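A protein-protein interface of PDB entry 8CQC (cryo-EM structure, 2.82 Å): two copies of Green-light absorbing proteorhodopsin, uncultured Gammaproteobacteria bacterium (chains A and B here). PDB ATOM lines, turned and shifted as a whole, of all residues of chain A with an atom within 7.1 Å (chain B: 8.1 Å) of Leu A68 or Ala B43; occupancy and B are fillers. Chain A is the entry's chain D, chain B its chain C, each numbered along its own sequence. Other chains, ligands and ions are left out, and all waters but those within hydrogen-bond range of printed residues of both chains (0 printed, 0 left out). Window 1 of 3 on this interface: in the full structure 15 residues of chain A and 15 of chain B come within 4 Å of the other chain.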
ATOM      1  N   THR A  45      22.335   6.528   7.432  1.00  0.00           N
ATOM      2  CA  THR A  45      21.221   7.113   6.695  1.00  0.00           C
ATOM      3  C   THR A  45      21.222   6.639   5.251  1.00  0.00           C
ATOM      4  O   THR A  45      20.197   6.173   4.733  1.00  0.00           O
ATOM      5  CB  THR A  45      21.303   8.638   6.754  1.00  0.00           C
ATOM      6  OG1 THR A  45      21.310   9.063   8.120  1.00  0.00           O
ATOM      7  CG2 THR A  45      20.126   9.266   6.041  1.00  0.00           C
ATOM      8  N   PHE A  48      20.364   2.825   5.056  1.00  0.00           N
ATOM      9  CA  PHE A  48      18.964   2.485   5.286  1.00  0.00           C
ATOM     10  C   PHE A  48      18.083   2.950   4.136  1.00  0.00           C
ATOM     11  O   PHE A  48      17.100   2.282   3.797  1.00  0.00           O
ATOM     12  CB  PHE A  48      18.476   3.090   6.600  1.00  0.00           C
ATOM     13  CG  PHE A  48      19.095   2.476   7.815  1.00  0.00           C
ATOM     14  CD1 PHE A  48      19.328   1.120   7.874  1.00  0.00           C
ATOM     15  CD2 PHE A  48      19.450   3.258   8.897  1.00  0.00           C
ATOM     16  CE1 PHE A  48      19.901   0.559   8.985  1.00  0.00           C
ATOM     17  CE2 PHE A  48      20.023   2.698  10.012  1.00  0.00           C
ATOM     18  CZ  PHE A  48      20.251   1.351  10.052  1.00  0.00           C
ATOM     19  N   PHE A  49      18.396   4.100   3.536  1.00  0.00           N
ATOM     20  CA  PHE A  49      17.595   4.543   2.401  1.00  0.00           C
ATOM     21  C   PHE A  49      17.883   3.724   1.152  1.00  0.00           C
ATOM     22  O   PHE A  49      17.015   3.598   0.283  1.00  0.00           O
ATOM     23  CB  PHE A  49      17.830   6.027   2.135  1.00  0.00           C
ATOM     24  CG  PHE A  49      17.085   6.927   3.067  1.00  0.00           C
ATOM     25  CD1 PHE A  49      15.804   6.610   3.473  1.00  0.00           C
ATOM     26  CD2 PHE A  49      17.666   8.081   3.549  1.00  0.00           C
ATOM     27  CE1 PHE A  49      15.120   7.429   4.332  1.00  0.00           C
ATOM     28  CE2 PHE A  49      16.979   8.906   4.408  1.00  0.00           C
ATOM     29  CZ  PHE A  49      15.708   8.578   4.800  1.00  0.00           C
ATOM     30  N   THR A  61       8.708   0.977   4.888  1.00  0.00           N
ATOM     31  CA  THR A  61       8.508   2.074   5.824  1.00  0.00           C
ATOM     32  C   THR A  61       9.438   1.921   7.013  1.00  0.00           C
ATOM     33  O   THR A  61      10.091   2.879   7.424  1.00  0.00           O
ATOM     34  CB  THR A  61       7.059   2.126   6.332  1.00  0.00           C
ATOM     35  OG1 THR A  61       6.164   2.185   5.217  1.00  0.00           O
ATOM     36  CG2 THR A  61       6.848   3.350   7.211  1.00  0.00           C
ATOM     37  N   SER A  62       9.503   0.714   7.565  1.00  0.00           N
ATOM     38  CA  SER A  62      10.389   0.468   8.692  1.00  0.00           C
ATOM     39  C   SER A  62      11.784   0.970   8.362  1.00  0.00           C
ATOM     40  O   SER A  62      12.386   1.705   9.143  1.00  0.00           O
ATOM     41  CB  SER A  62      10.425  -1.022   9.035  1.00  0.00           C
ATOM     42  OG  SER A  62       9.138  -1.494   9.393  1.00  0.00           O
ATOM     43  N   LEU A  63      12.304   0.580   7.189  1.00  0.00           N
ATOM     44  CA  LEU A  63      13.637   1.022   6.789  1.00  0.00           C
ATOM     45  C   LEU A  63      13.673   2.527   6.542  1.00  0.00           C
ATOM     46  O   LEU A  63      14.673   3.192   6.847  1.00  0.00           O
ATOM     47  CB  LEU A  63      14.106   0.250   5.558  1.00  0.00           C
ATOM     48  CG  LEU A  63      15.015  -0.942   5.873  1.00  0.00           C
ATOM     49  CD1 LEU A  63      14.283  -1.986   6.694  1.00  0.00           C
ATOM     50  CD2 LEU A  63      15.560  -1.553   4.604  1.00  0.00           C
ATOM     51  N   THR A  64      12.574   3.093   5.959  1.00  0.00           N
ATOM     52  CA  THR A  64      12.510   4.527   5.717  1.00  0.00           C
ATOM     53  C   THR A  64      12.724   5.268   7.024  1.00  0.00           C
ATOM     54  O   THR A  64      13.530   6.197   7.093  1.00  0.00           O
ATOM     55  CB  THR A  64      11.158   4.937   5.108  1.00  0.00           C
ATOM     56  OG1 THR A  64      10.919   4.182   3.913  1.00  0.00           O
ATOM     57  CG2 THR A  64      11.150   6.422   4.778  1.00  0.00           C
ATOM     58  N   VAL A  65      12.010   4.853   8.064  1.00  0.00           N
ATOM     59  CA  VAL A  65      12.142   5.502   9.364  1.00  0.00           C
ATOM     60  C   VAL A  65      13.552   5.357   9.912  1.00  0.00           C
ATOM     61  O   VAL A  65      14.163   6.341  10.330  1.00  0.00           O
ATOM     62  CB  VAL A  65      11.151   4.911  10.381  1.00  0.00           C
ATOM     63  CG1 VAL A  65      11.383   5.510  11.760  1.00  0.00           C
ATOM     64  CG2 VAL A  65       9.722   5.148   9.919  1.00  0.00           C
ATOM     65  N   SER A  66      14.074   4.136   9.908  1.00  0.00           N
ATOM     66  CA  SER A  66      15.430   3.910  10.388  1.00  0.00           C
ATOM     67  C   SER A  66      16.361   4.900   9.723  1.00  0.00           C
ATOM     68  O   SER A  66      17.315   5.379  10.337  1.00  0.00           O
ATOM     69  CB  SER A  66      15.874   2.481  10.088  1.00  0.00           C
ATOM     70  OG  SER A  66      14.981   1.539  10.656  1.00  0.00           O
ATOM     71  N   GLY A  67      16.087   5.218   8.469  1.00  0.00           N
ATOM     72  CA  GLY A  67      16.916   6.158   7.736  1.00  0.00           C
ATOM     73  C   GLY A  67      16.646   7.579   8.176  1.00  0.00           C
ATOM     74  O   GLY A  67      17.578   8.352   8.404  1.00  0.00           O
ATOM     75  N   LEU A  68      15.372   7.930   8.303  1.00  0.00           N
ATOM     76  CA  LEU A  68      15.011   9.274   8.732  1.00  0.00           C
ATOM     77  C   LEU A  68      15.578   9.561  10.111  1.00  0.00           C
ATOM     78  O   LEU A  68      16.157  10.623  10.340  1.00  0.00           O
ATOM     79  CB  LEU A  68      13.492   9.441   8.742  1.00  0.00           C
ATOM     80  CG  LEU A  68      12.802   9.375   7.379  1.00  0.00           C
ATOM     81  CD1 LEU A  68      11.293   9.279   7.540  1.00  0.00           C
ATOM     82  CD2 LEU A  68      13.184  10.568   6.515  1.00  0.00           C
ATOM     83  N   VAL A  69      15.424   8.614  11.030  1.00  0.00           N
ATOM     84  CA  VAL A  69      15.968   8.791  12.371  1.00  0.00           C
ATOM     85  C   VAL A  69      17.437   9.170  12.289  1.00  0.00           C
ATOM     86  O   VAL A  69      17.845  10.212  12.801  1.00  0.00           O
ATOM     87  CB  VAL A  69      15.819   7.518  13.224  1.00  0.00           C
ATOM     88  CG1 VAL A  69      16.649   7.630  14.494  1.00  0.00           C
ATOM     89  CG2 VAL A  69      14.356   7.268  13.557  1.00  0.00           C
ATOM     90  N   THR A  70      18.247   8.302  11.645  1.00  0.00           N
ATOM     91  CA  THR A  70      19.678   8.574  11.523  1.00  0.00           C
ATOM     92  C   THR A  70      19.940   9.901  10.815  1.00  0.00           C
ATOM     93  O   THR A  70      20.865  10.634  11.180  1.00  0.00           O
ATOM     94  CB  THR A  70      20.385   7.429  10.803  1.00  0.00           C
ATOM     95  OG1 THR A  70      19.607   7.017   9.675  1.00  0.00           O
ATOM     96  CG2 THR A  70      20.575   6.253  11.739  1.00  0.00           C
ATOM     97  N   GLY A  71      19.133  10.233   9.806  1.00  0.00           N
ATOM     98  CA  GLY A  71      19.321  11.489   9.099  1.00  0.00           C
ATOM     99  C   GLY A  71      19.038  12.706   9.956  1.00  0.00           C
ATOM    100  O   GLY A  71      19.776  13.691   9.907  1.00  0.00           O
ATOM    101  N   ILE A  72      17.960  12.663  10.710  1.00  0.00           N
ATOM    102  CA  ILE A  72      17.664  13.768  11.609  1.00  0.00           C
ATOM    103  C   ILE A  72      18.813  13.905  12.586  1.00  0.00           C
ATOM    104  O   ILE A  72      19.333  15.002  12.795  1.00  0.00           O
ATOM    105  CB  ILE A  72      16.360  13.539  12.387  1.00  0.00           C
ATOM    106  CG1 ILE A  72      15.167  13.510  11.432  1.00  0.00           C
ATOM    107  CG2 ILE A  72      16.167  14.622  13.437  1.00  0.00           C
ATOM    108  CD1 ILE A  72      13.846  13.238  12.116  1.00  0.00           C
ATOM    109  N   ALA A  73      19.217  12.788  13.180  1.00  0.00           N
ATOM    110  CA  ALA A  73      20.334  12.810  14.110  1.00  0.00           C
ATOM    111  C   ALA A  73      21.516  13.536  13.488  1.00  0.00           C
ATOM    112  O   ALA A  73      22.025  14.503  14.053  1.00  0.00           O
ATOM    113  CB  ALA A  73      20.724  11.397  14.506  1.00  0.00           C
ATOM    114  N   PHE A  74      21.964  13.076  12.326  1.00  0.00           N
ATOM    115  CA  PHE A  74      23.083  13.720  11.644  1.00  0.00           C
ATOM    116  C   PHE A  74      22.869  15.223  11.552  1.00  0.00           C
ATOM    117  O   PHE A  74      23.732  15.998  11.956  1.00  0.00           O
ATOM    118  CB  PHE A  74      23.243  13.121  10.247  1.00  0.00           C
ATOM    119  CG  PHE A  74      24.344  13.740   9.437  1.00  0.00           C
ATOM    120  CD1 PHE A  74      24.106  14.860   8.659  1.00  0.00           C
ATOM    121  CD2 PHE A  74      25.614  13.192   9.441  1.00  0.00           C
ATOM    122  CE1 PHE A  74      25.117  15.427   7.907  1.00  0.00           C
ATOM    123  CE2 PHE A  74      26.629  13.752   8.690  1.00  0.00           C
ATOM    124  CZ  PHE A  74      26.381  14.872   7.923  1.00  0.00           C
ATOM    125  N   LEU A 101      12.241  14.758  18.085  1.00  0.00           N
ATOM    126  CA  LEU A 101      11.964  14.309  16.726  1.00  0.00           C
ATOM    127  C   LEU A 101      12.247  12.827  16.495  1.00  0.00           C
ATOM    128  O   LEU A 101      11.530  12.191  15.715  1.00  0.00           O
ATOM    129  CB  LEU A 101      12.763  15.139  15.724  1.00  0.00           C
ATOM    130  CG  LEU A 101      12.225  16.549  15.499  1.00  0.00           C
ATOM    131  CD1 LEU A 101      13.180  17.336  14.643  1.00  0.00           C
ATOM    132  CD2 LEU A 101      10.853  16.496  14.857  1.00  0.00           C
ATOM    133  N   THR A 102      13.260  12.254  17.145  1.00  0.00           N
ATOM    134  CA  THR A 102      13.705  10.901  16.823  1.00  0.00           C
ATOM    135  C   THR A 102      13.148   9.826  17.748  1.00  0.00           C
ATOM    136  O   THR A 102      12.870   8.719  17.286  1.00  0.00           O
ATOM    137  CB  THR A 102      15.235  10.823  16.838  1.00  0.00           C
ATOM    138  OG1 THR A 102      15.726  11.268  18.107  1.00  0.00           O
ATOM    139  CG2 THR A 102      15.825  11.682  15.738  1.00  0.00           C
ATOM    140  N   LEU A 105       9.877   8.318  16.544  1.00  0.00           N
ATOM    141  CA  LEU A 105      10.051   7.411  15.413  1.00  0.00           C
ATOM    142  C   LEU A 105      10.681   6.091  15.847  1.00  0.00           C
ATOM    143  O   LEU A 105      10.282   5.016  15.379  1.00  0.00           O
ATOM    144  CB  LEU A 105      10.895   8.082  14.333  1.00  0.00           C
ATOM    145  CG  LEU A 105      10.384   9.395  13.737  1.00  0.00           C
ATOM    146  CD1 LEU A 105      11.414   9.988  12.796  1.00  0.00           C
ATOM    147  CD2 LEU A 105       9.076   9.176  13.014  1.00  0.00           C
ATOM    148  N   LEU B  36      12.657  23.012  14.963  1.00  0.00           N
ATOM    149  CA  LEU B  36      11.839  21.807  15.031  1.00  0.00           C
ATOM    150  C   LEU B  36      11.036  21.615  13.750  1.00  0.00           C
ATOM    151  O   LEU B  36      11.050  20.534  13.148  1.00  0.00           O
ATOM    152  CB  LEU B  36      10.914  21.893  16.244  1.00  0.00           C
ATOM    153  CG  LEU B  36      10.257  20.621  16.769  1.00  0.00           C
ATOM    154  CD1 LEU B  36      11.291  19.721  17.413  1.00  0.00           C
ATOM    155  CD2 LEU B  36       9.163  20.975  17.756  1.00  0.00           C
ATOM    156  N   VAL B  37      10.348  22.667  13.303  1.00  0.00           N
ATOM    157  CA  VAL B  37       9.517  22.581  12.109  1.00  0.00           C
ATOM    158  C   VAL B  37      10.375  22.387  10.868  1.00  0.00           C
ATOM    159  O   VAL B  37       9.991  21.664   9.948  1.00  0.00           O
ATOM    160  CB  VAL B  37       8.618  23.825  11.995  1.00  0.00           C
ATOM    161  CG1 VAL B  37       7.857  23.816  10.686  1.00  0.00           C
ATOM    162  CG2 VAL B  37       7.647  23.879  13.157  1.00  0.00           C
ATOM    163  N   THR B  38      11.548  23.019  10.817  1.00  0.00           N
ATOM    164  CA  THR B  38      12.422  22.865   9.660  1.00  0.00           C
ATOM    165  C   THR B  38      12.896  21.423   9.515  1.00  0.00           C
ATOM    166  O   THR B  38      12.843  20.840   8.423  1.00  0.00           O
ATOM    167  CB  THR B  38      13.608  23.819   9.791  1.00  0.00           C
ATOM    168  OG1 THR B  38      13.129  25.167   9.825  1.00  0.00           O
ATOM    169  CG2 THR B  38      14.554  23.662   8.631  1.00  0.00           C
ATOM    170  N   ALA B  39      13.354  20.825  10.617  1.00  0.00           N
ATOM    171  CA  ALA B  39      13.791  19.434  10.568  1.00  0.00           C
ATOM    172  C   ALA B  39      12.629  18.497  10.261  1.00  0.00           C
ATOM    173  O   ALA B  39      12.787  17.537   9.495  1.00  0.00           O
ATOM    174  CB  ALA B  39      14.465  19.052  11.882  1.00  0.00           C
ATOM    175  N   ALA B  40      11.455  18.757  10.844  1.00  0.00           N
ATOM    176  CA  ALA B  40      10.293  17.922  10.565  1.00  0.00           C
ATOM    177  C   ALA B  40       9.875  18.017   9.102  1.00  0.00           C
ATOM    178  O   ALA B  40       9.487  17.014   8.497  1.00  0.00           O
ATOM    179  CB  ALA B  40       9.137  18.311  11.483  1.00  0.00           C
ATOM    180  N   LEU B  41       9.949  19.213   8.514  1.00  0.00           N
ATOM    181  CA  LEU B  41       9.597  19.374   7.107  1.00  0.00           C
ATOM    182  C   LEU B  41      10.598  18.675   6.197  1.00  0.00           C
ATOM    183  O   LEU B  41      10.207  18.078   5.191  1.00  0.00           O
ATOM    184  CB  LEU B  41       9.499  20.855   6.752  1.00  0.00           C
ATOM    185  CG  LEU B  41       8.290  21.629   7.271  1.00  0.00           C
ATOM    186  CD1 LEU B  41       8.482  23.106   7.017  1.00  0.00           C
ATOM    187  CD2 LEU B  41       7.012  21.140   6.623  1.00  0.00           C
ATOM    188  N   LEU B  42      11.883  18.718   6.567  1.00  0.00           N
ATOM    189  CA  LEU B  42      12.885  18.023   5.774  1.00  0.00           C
ATOM    190  C   LEU B  42      12.613  16.530   5.819  1.00  0.00           C
ATOM    191  O   LEU B  42      12.588  15.868   4.781  1.00  0.00           O
ATOM    192  CB  LEU B  42      14.281  18.328   6.308  1.00  0.00           C
ATOM    193  CG  LEU B  42      15.458  17.910   5.429  1.00  0.00           C
ATOM    194  CD1 LEU B  42      15.313  18.511   4.039  1.00  0.00           C
ATOM    195  CD2 LEU B  42      16.772  18.336   6.068  1.00  0.00           C
ATOM    196  N   ALA B  43      12.410  15.999   7.015  1.00  0.00           N
ATOM    197  CA  ALA B  43      12.153  14.574   7.181  1.00  0.00           C
ATOM    198  C   ALA B  43      10.888  14.152   6.446  1.00  0.00           C
ATOM    199  O   ALA B  43      10.851  13.083   5.831  1.00  0.00           O
ATOM    200  CB  ALA B  43      12.057  14.228   8.665  1.00  0.00           C
ATOM    201  N   SER B  44       9.842  14.978   6.499  1.00  0.00           N
ATOM    202  CA  SER B  44       8.604  14.665   5.792  1.00  0.00           C
ATOM    203  C   SER B  44       8.800  14.685   4.283  1.00  0.00           C
ATOM    204  O   SER B  44       8.225  13.860   3.571  1.00  0.00           O
ATOM    205  CB  SER B  44       7.510  15.646   6.198  1.00  0.00           C
ATOM    206  OG  SER B  44       7.304  15.621   7.594  1.00  0.00           O
ATOM    207  N   THR B  45       9.588  15.635   3.775  1.00  0.00           N
ATOM    208  CA  THR B  45       9.889  15.667   2.348  1.00  0.00           C
ATOM    209  C   THR B  45      10.558  14.374   1.907  1.00  0.00           C
ATOM    210  O   THR B  45      10.145  13.747   0.921  1.00  0.00           O
ATOM    211  CB  THR B  45      10.789  16.861   2.034  1.00  0.00           C
ATOM    212  OG1 THR B  45      10.122  18.070   2.403  1.00  0.00           O
ATOM    213  CG2 THR B  45      11.125  16.907   0.560  1.00  0.00           C
ATOM    214  N   VAL B  46      11.595  13.957   2.638  1.00  0.00           N
ATOM    215  CA  VAL B  46      12.286  12.719   2.284  1.00  0.00           C
ATOM    216  C   VAL B  46      11.342  11.528   2.402  1.00  0.00           C
ATOM    217  O   VAL B  46      11.330  10.643   1.541  1.00  0.00           O
ATOM    218  CB  VAL B  46      13.546  12.538   3.149  1.00  0.00           C
ATOM    219  CG1 VAL B  46      14.265  11.264   2.762  1.00  0.00           C
ATOM    220  CG2 VAL B  46      14.465  13.731   2.994  1.00  0.00           C
ATOM    221  N   PHE B  47      10.528  11.495   3.460  1.00  0.00           N
ATOM    222  CA  PHE B  47       9.605  10.386   3.674  1.00  0.00           C
ATOM    223  C   PHE B  47       8.607  10.268   2.529  1.00  0.00           C
ATOM    224  O   PHE B  47       8.348   9.169   2.031  1.00  0.00           O
ATOM    225  CB  PHE B  47       8.882  10.577   5.008  1.00  0.00           C
ATOM    226  CG  PHE B  47       7.913   9.481   5.350  1.00  0.00           C
ATOM    227  CD1 PHE B  47       8.344   8.329   5.982  1.00  0.00           C
ATOM    228  CD2 PHE B  47       6.567   9.614   5.063  1.00  0.00           C
ATOM    229  CE1 PHE B  47       7.453   7.328   6.303  1.00  0.00           C
ATOM    230  CE2 PHE B  47       5.676   8.616   5.380  1.00  0.00           C
ATOM    231  CZ  PHE B  47       6.119   7.475   6.002  1.00  0.00           C
ATOM    232  N   PHE B  48       8.035  11.394   2.097  1.00  0.00           N
ATOM    233  CA  PHE B  48       7.040  11.361   1.029  1.00  0.00           C
ATOM    234  C   PHE B  48       7.668  10.998  -0.306  1.00  0.00           C
ATOM    235  O   PHE B  48       7.063  10.270  -1.101  1.00  0.00           O
ATOM    236  CB  PHE B  48       6.324  12.704   0.924  1.00  0.00           C
ATOM    237  CG  PHE B  48       5.453  13.017   2.098  1.00  0.00           C
ATOM    238  CD1 PHE B  48       4.748  12.018   2.732  1.00  0.00           C
ATOM    239  CD2 PHE B  48       5.347  14.310   2.573  1.00  0.00           C
ATOM    240  CE1 PHE B  48       3.955  12.302   3.813  1.00  0.00           C
ATOM    241  CE2 PHE B  48       4.553  14.599   3.656  1.00  0.00           C
ATOM    242  CZ  PHE B  48       3.859  13.594   4.277  1.00  0.00           C
ATOM    243  N   PHE B  49       8.870  11.502  -0.587  1.00  0.00           N
ATOM    244  CA  PHE B  49       9.498  11.155  -1.856  1.00  0.00           C
ATOM    245  C   PHE B  49       9.988   9.715  -1.868  1.00  0.00           C
ATOM    246  O   PHE B  49      10.117   9.116  -2.940  1.00  0.00           O
ATOM    247  CB  PHE B  49      10.642  12.117  -2.159  1.00  0.00           C
ATOM    248  CG  PHE B  49      10.189  13.432  -2.713  1.00  0.00           C
ATOM    249  CD1 PHE B  49       9.183  13.488  -3.657  1.00  0.00           C
ATOM    250  CD2 PHE B  49      10.759  14.613  -2.284  1.00  0.00           C
ATOM    251  CE1 PHE B  49       8.763  14.690  -4.164  1.00  0.00           C
ATOM    252  CE2 PHE B  49      10.340  15.818  -2.790  1.00  0.00           C
ATOM    253  CZ  PHE B  49       9.342  15.857  -3.731  1.00  0.00           C
ATOM    254  N   VAL B  50      10.251   9.139  -0.697  1.00  0.00           N
ATOM    255  CA  VAL B  50      10.778   7.782  -0.633  1.00  0.00           C
ATOM    256  C   VAL B  50       9.652   6.754  -0.606  1.00  0.00           C
ATOM    257  O   VAL B  50       9.765   5.682  -1.207  1.00  0.00           O
ATOM    258  CB  VAL B  50      11.712   7.655   0.584  1.00  0.00           C
ATOM    259  CG1 VAL B  50      11.800   6.230   1.056  1.00  0.00           C
ATOM    260  CG2 VAL B  50      13.093   8.172   0.235  1.00  0.00           C
ATOM    261  N   GLU B  51       8.542   7.066   0.060  1.00  0.00           N
ATOM    262  CA  GLU B  51       7.452   6.118   0.239  1.00  0.00           C
ATOM    263  C   GLU B  51       6.559   5.976  -0.983  1.00  0.00           C
ATOM    264  O   GLU B  51       5.508   5.337  -0.883  1.00  0.00           O
ATOM    265  CB  GLU B  51       6.609   6.518   1.449  1.00  0.00           C
ATOM    266  CG  GLU B  51       7.271   6.236   2.784  1.00  0.00           C
ATOM    267  CD  GLU B  51       7.422   4.758   3.062  1.00  0.00           C
ATOM    268  OE1 GLU B  51       8.397   4.149   2.579  1.00  0.00           O
ATOM    269  OE2 GLU B  51       6.557   4.196   3.759  1.00  0.00           O
ATOM    270  N   THR B  70       5.959  19.967   1.301  1.00  0.00           N
ATOM    271  CA  THR B  70       6.865  20.017   2.448  1.00  0.00           C
ATOM    272  C   THR B  70       8.245  20.535   2.050  1.00  0.00           C
ATOM    273  O   THR B  70       8.890  21.256   2.821  1.00  0.00           O
ATOM    274  CB  THR B  70       6.971  18.646   3.110  1.00  0.00           C
ATOM    275  OG1 THR B  70       7.202  17.647   2.115  1.00  0.00           O
ATOM    276  CG2 THR B  70       5.698  18.324   3.861  1.00  0.00           C
ATOM    277  N   PHE B  74      10.081  23.815   3.603  1.00  0.00           N
ATOM    278  CA  PHE B  74      11.433  23.803   4.153  1.00  0.00           C
ATOM    279  C   PHE B  74      12.283  24.897   3.530  1.00  0.00           C
ATOM    280  O   PHE B  74      12.881  25.701   4.242  1.00  0.00           O
ATOM    281  CB  PHE B  74      12.070  22.435   3.910  1.00  0.00           C
ATOM    282  CG  PHE B  74      13.483  22.320   4.402  1.00  0.00           C
ATOM    283  CD1 PHE B  74      14.547  22.682   3.591  1.00  0.00           C
ATOM    284  CD2 PHE B  74      13.751  21.834   5.669  1.00  0.00           C
ATOM    285  CE1 PHE B  74      15.848  22.571   4.040  1.00  0.00           C
ATOM    286  CE2 PHE B  74      15.050  21.718   6.123  1.00  0.00           C
ATOM    287  CZ  PHE B  74      16.101  22.088   5.308  1.00  0.00           C
ATOM    288  N   ILE B 233       2.401  18.341   7.428  1.00  0.00           N
ATOM    289  CA  ILE B 233       2.898  17.003   7.706  1.00  0.00           C
ATOM    290  C   ILE B 233       1.756  16.025   7.939  1.00  0.00           C
ATOM    291  O   ILE B 233       1.743  14.932   7.377  1.00  0.00           O
ATOM    292  CB  ILE B 233       3.877  17.036   8.900  1.00  0.00           C
ATOM    293  CG1 ILE B 233       5.045  17.973   8.588  1.00  0.00           C
ATOM    294  CG2 ILE B 233       4.388  15.647   9.208  1.00  0.00           C
ATOM    295  CD1 ILE B 233       5.915  18.280   9.771  1.00  0.00           C
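Leu A68 touches just these residues of chain B: Ala B43, Val B46 and Phe B47.
Printed residues of chain A within 4 Å of Ala B43: Leu A68 (3.5 Å).
No residue of chain B comes within 4 Å of Gly A67.
Of the printed residues of chain A, Val B46 touches Phe A49 (3.7 Å) and Leu A68 (3.9 Å).
Printed residues of chain B within 4 Å of Thr A61: Glu B51 (2.5 Å).
Of the printed residues of chain A, Phe B47 touches Thr A64 and Leu A68.
Of the printed residues of chain B, Leu A101 touches Leu B36 and Ala B39.
Val A69 touches none of the printed residues of chain B.
Ser A62 touches none of the printed residues of chain B.
The nearest residue of chain B that does not touch Leu A68 is Ser B44 (5.5 Å).
The nearest printed residue of chain B that does not touch Phe A49 is Val B50 (4.5 Å).
Hydrophobic or aromatic side chains of chain A that line the printed part of chain B: Phe A49, Leu A68 and Leu A101.
Among the printed residues, no Asp or Glu carboxylate lies within 4 Å of a Lys or Arg side-chain nitrogen of the other chain.
OG1 of Thr A64 sits at hydrogen-bond distance from OE1 of Glu B51 (2.9 Å).
OG1 of Thr A61 is in hydrogen-bond range of OE2 of Glu B51 (2.5 Å).
Among the printed residues, merely in contact across the chains: Leu A68 with Phe B47 (3.5 Å), Leu A101 with Ala B39 (3.5 Å), Leu A68 with Ala B43 (3.5 Å), Thr A64 with Phe B47 (3.6 Å), Thr A64 with Val B50 (3.6 Å), Phe A49 with Val B46 (3.7 Å), Leu A101 with Leu B36 (3.8 Å) and Leu A68 with Val B46 (3.9 Å).
Positions printed for both chains: 45, 48, 49, 70 and 74.
Of the 10 pairs that touch across the chains among the printed residues, none has its exchanged pair printed and touching as well.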
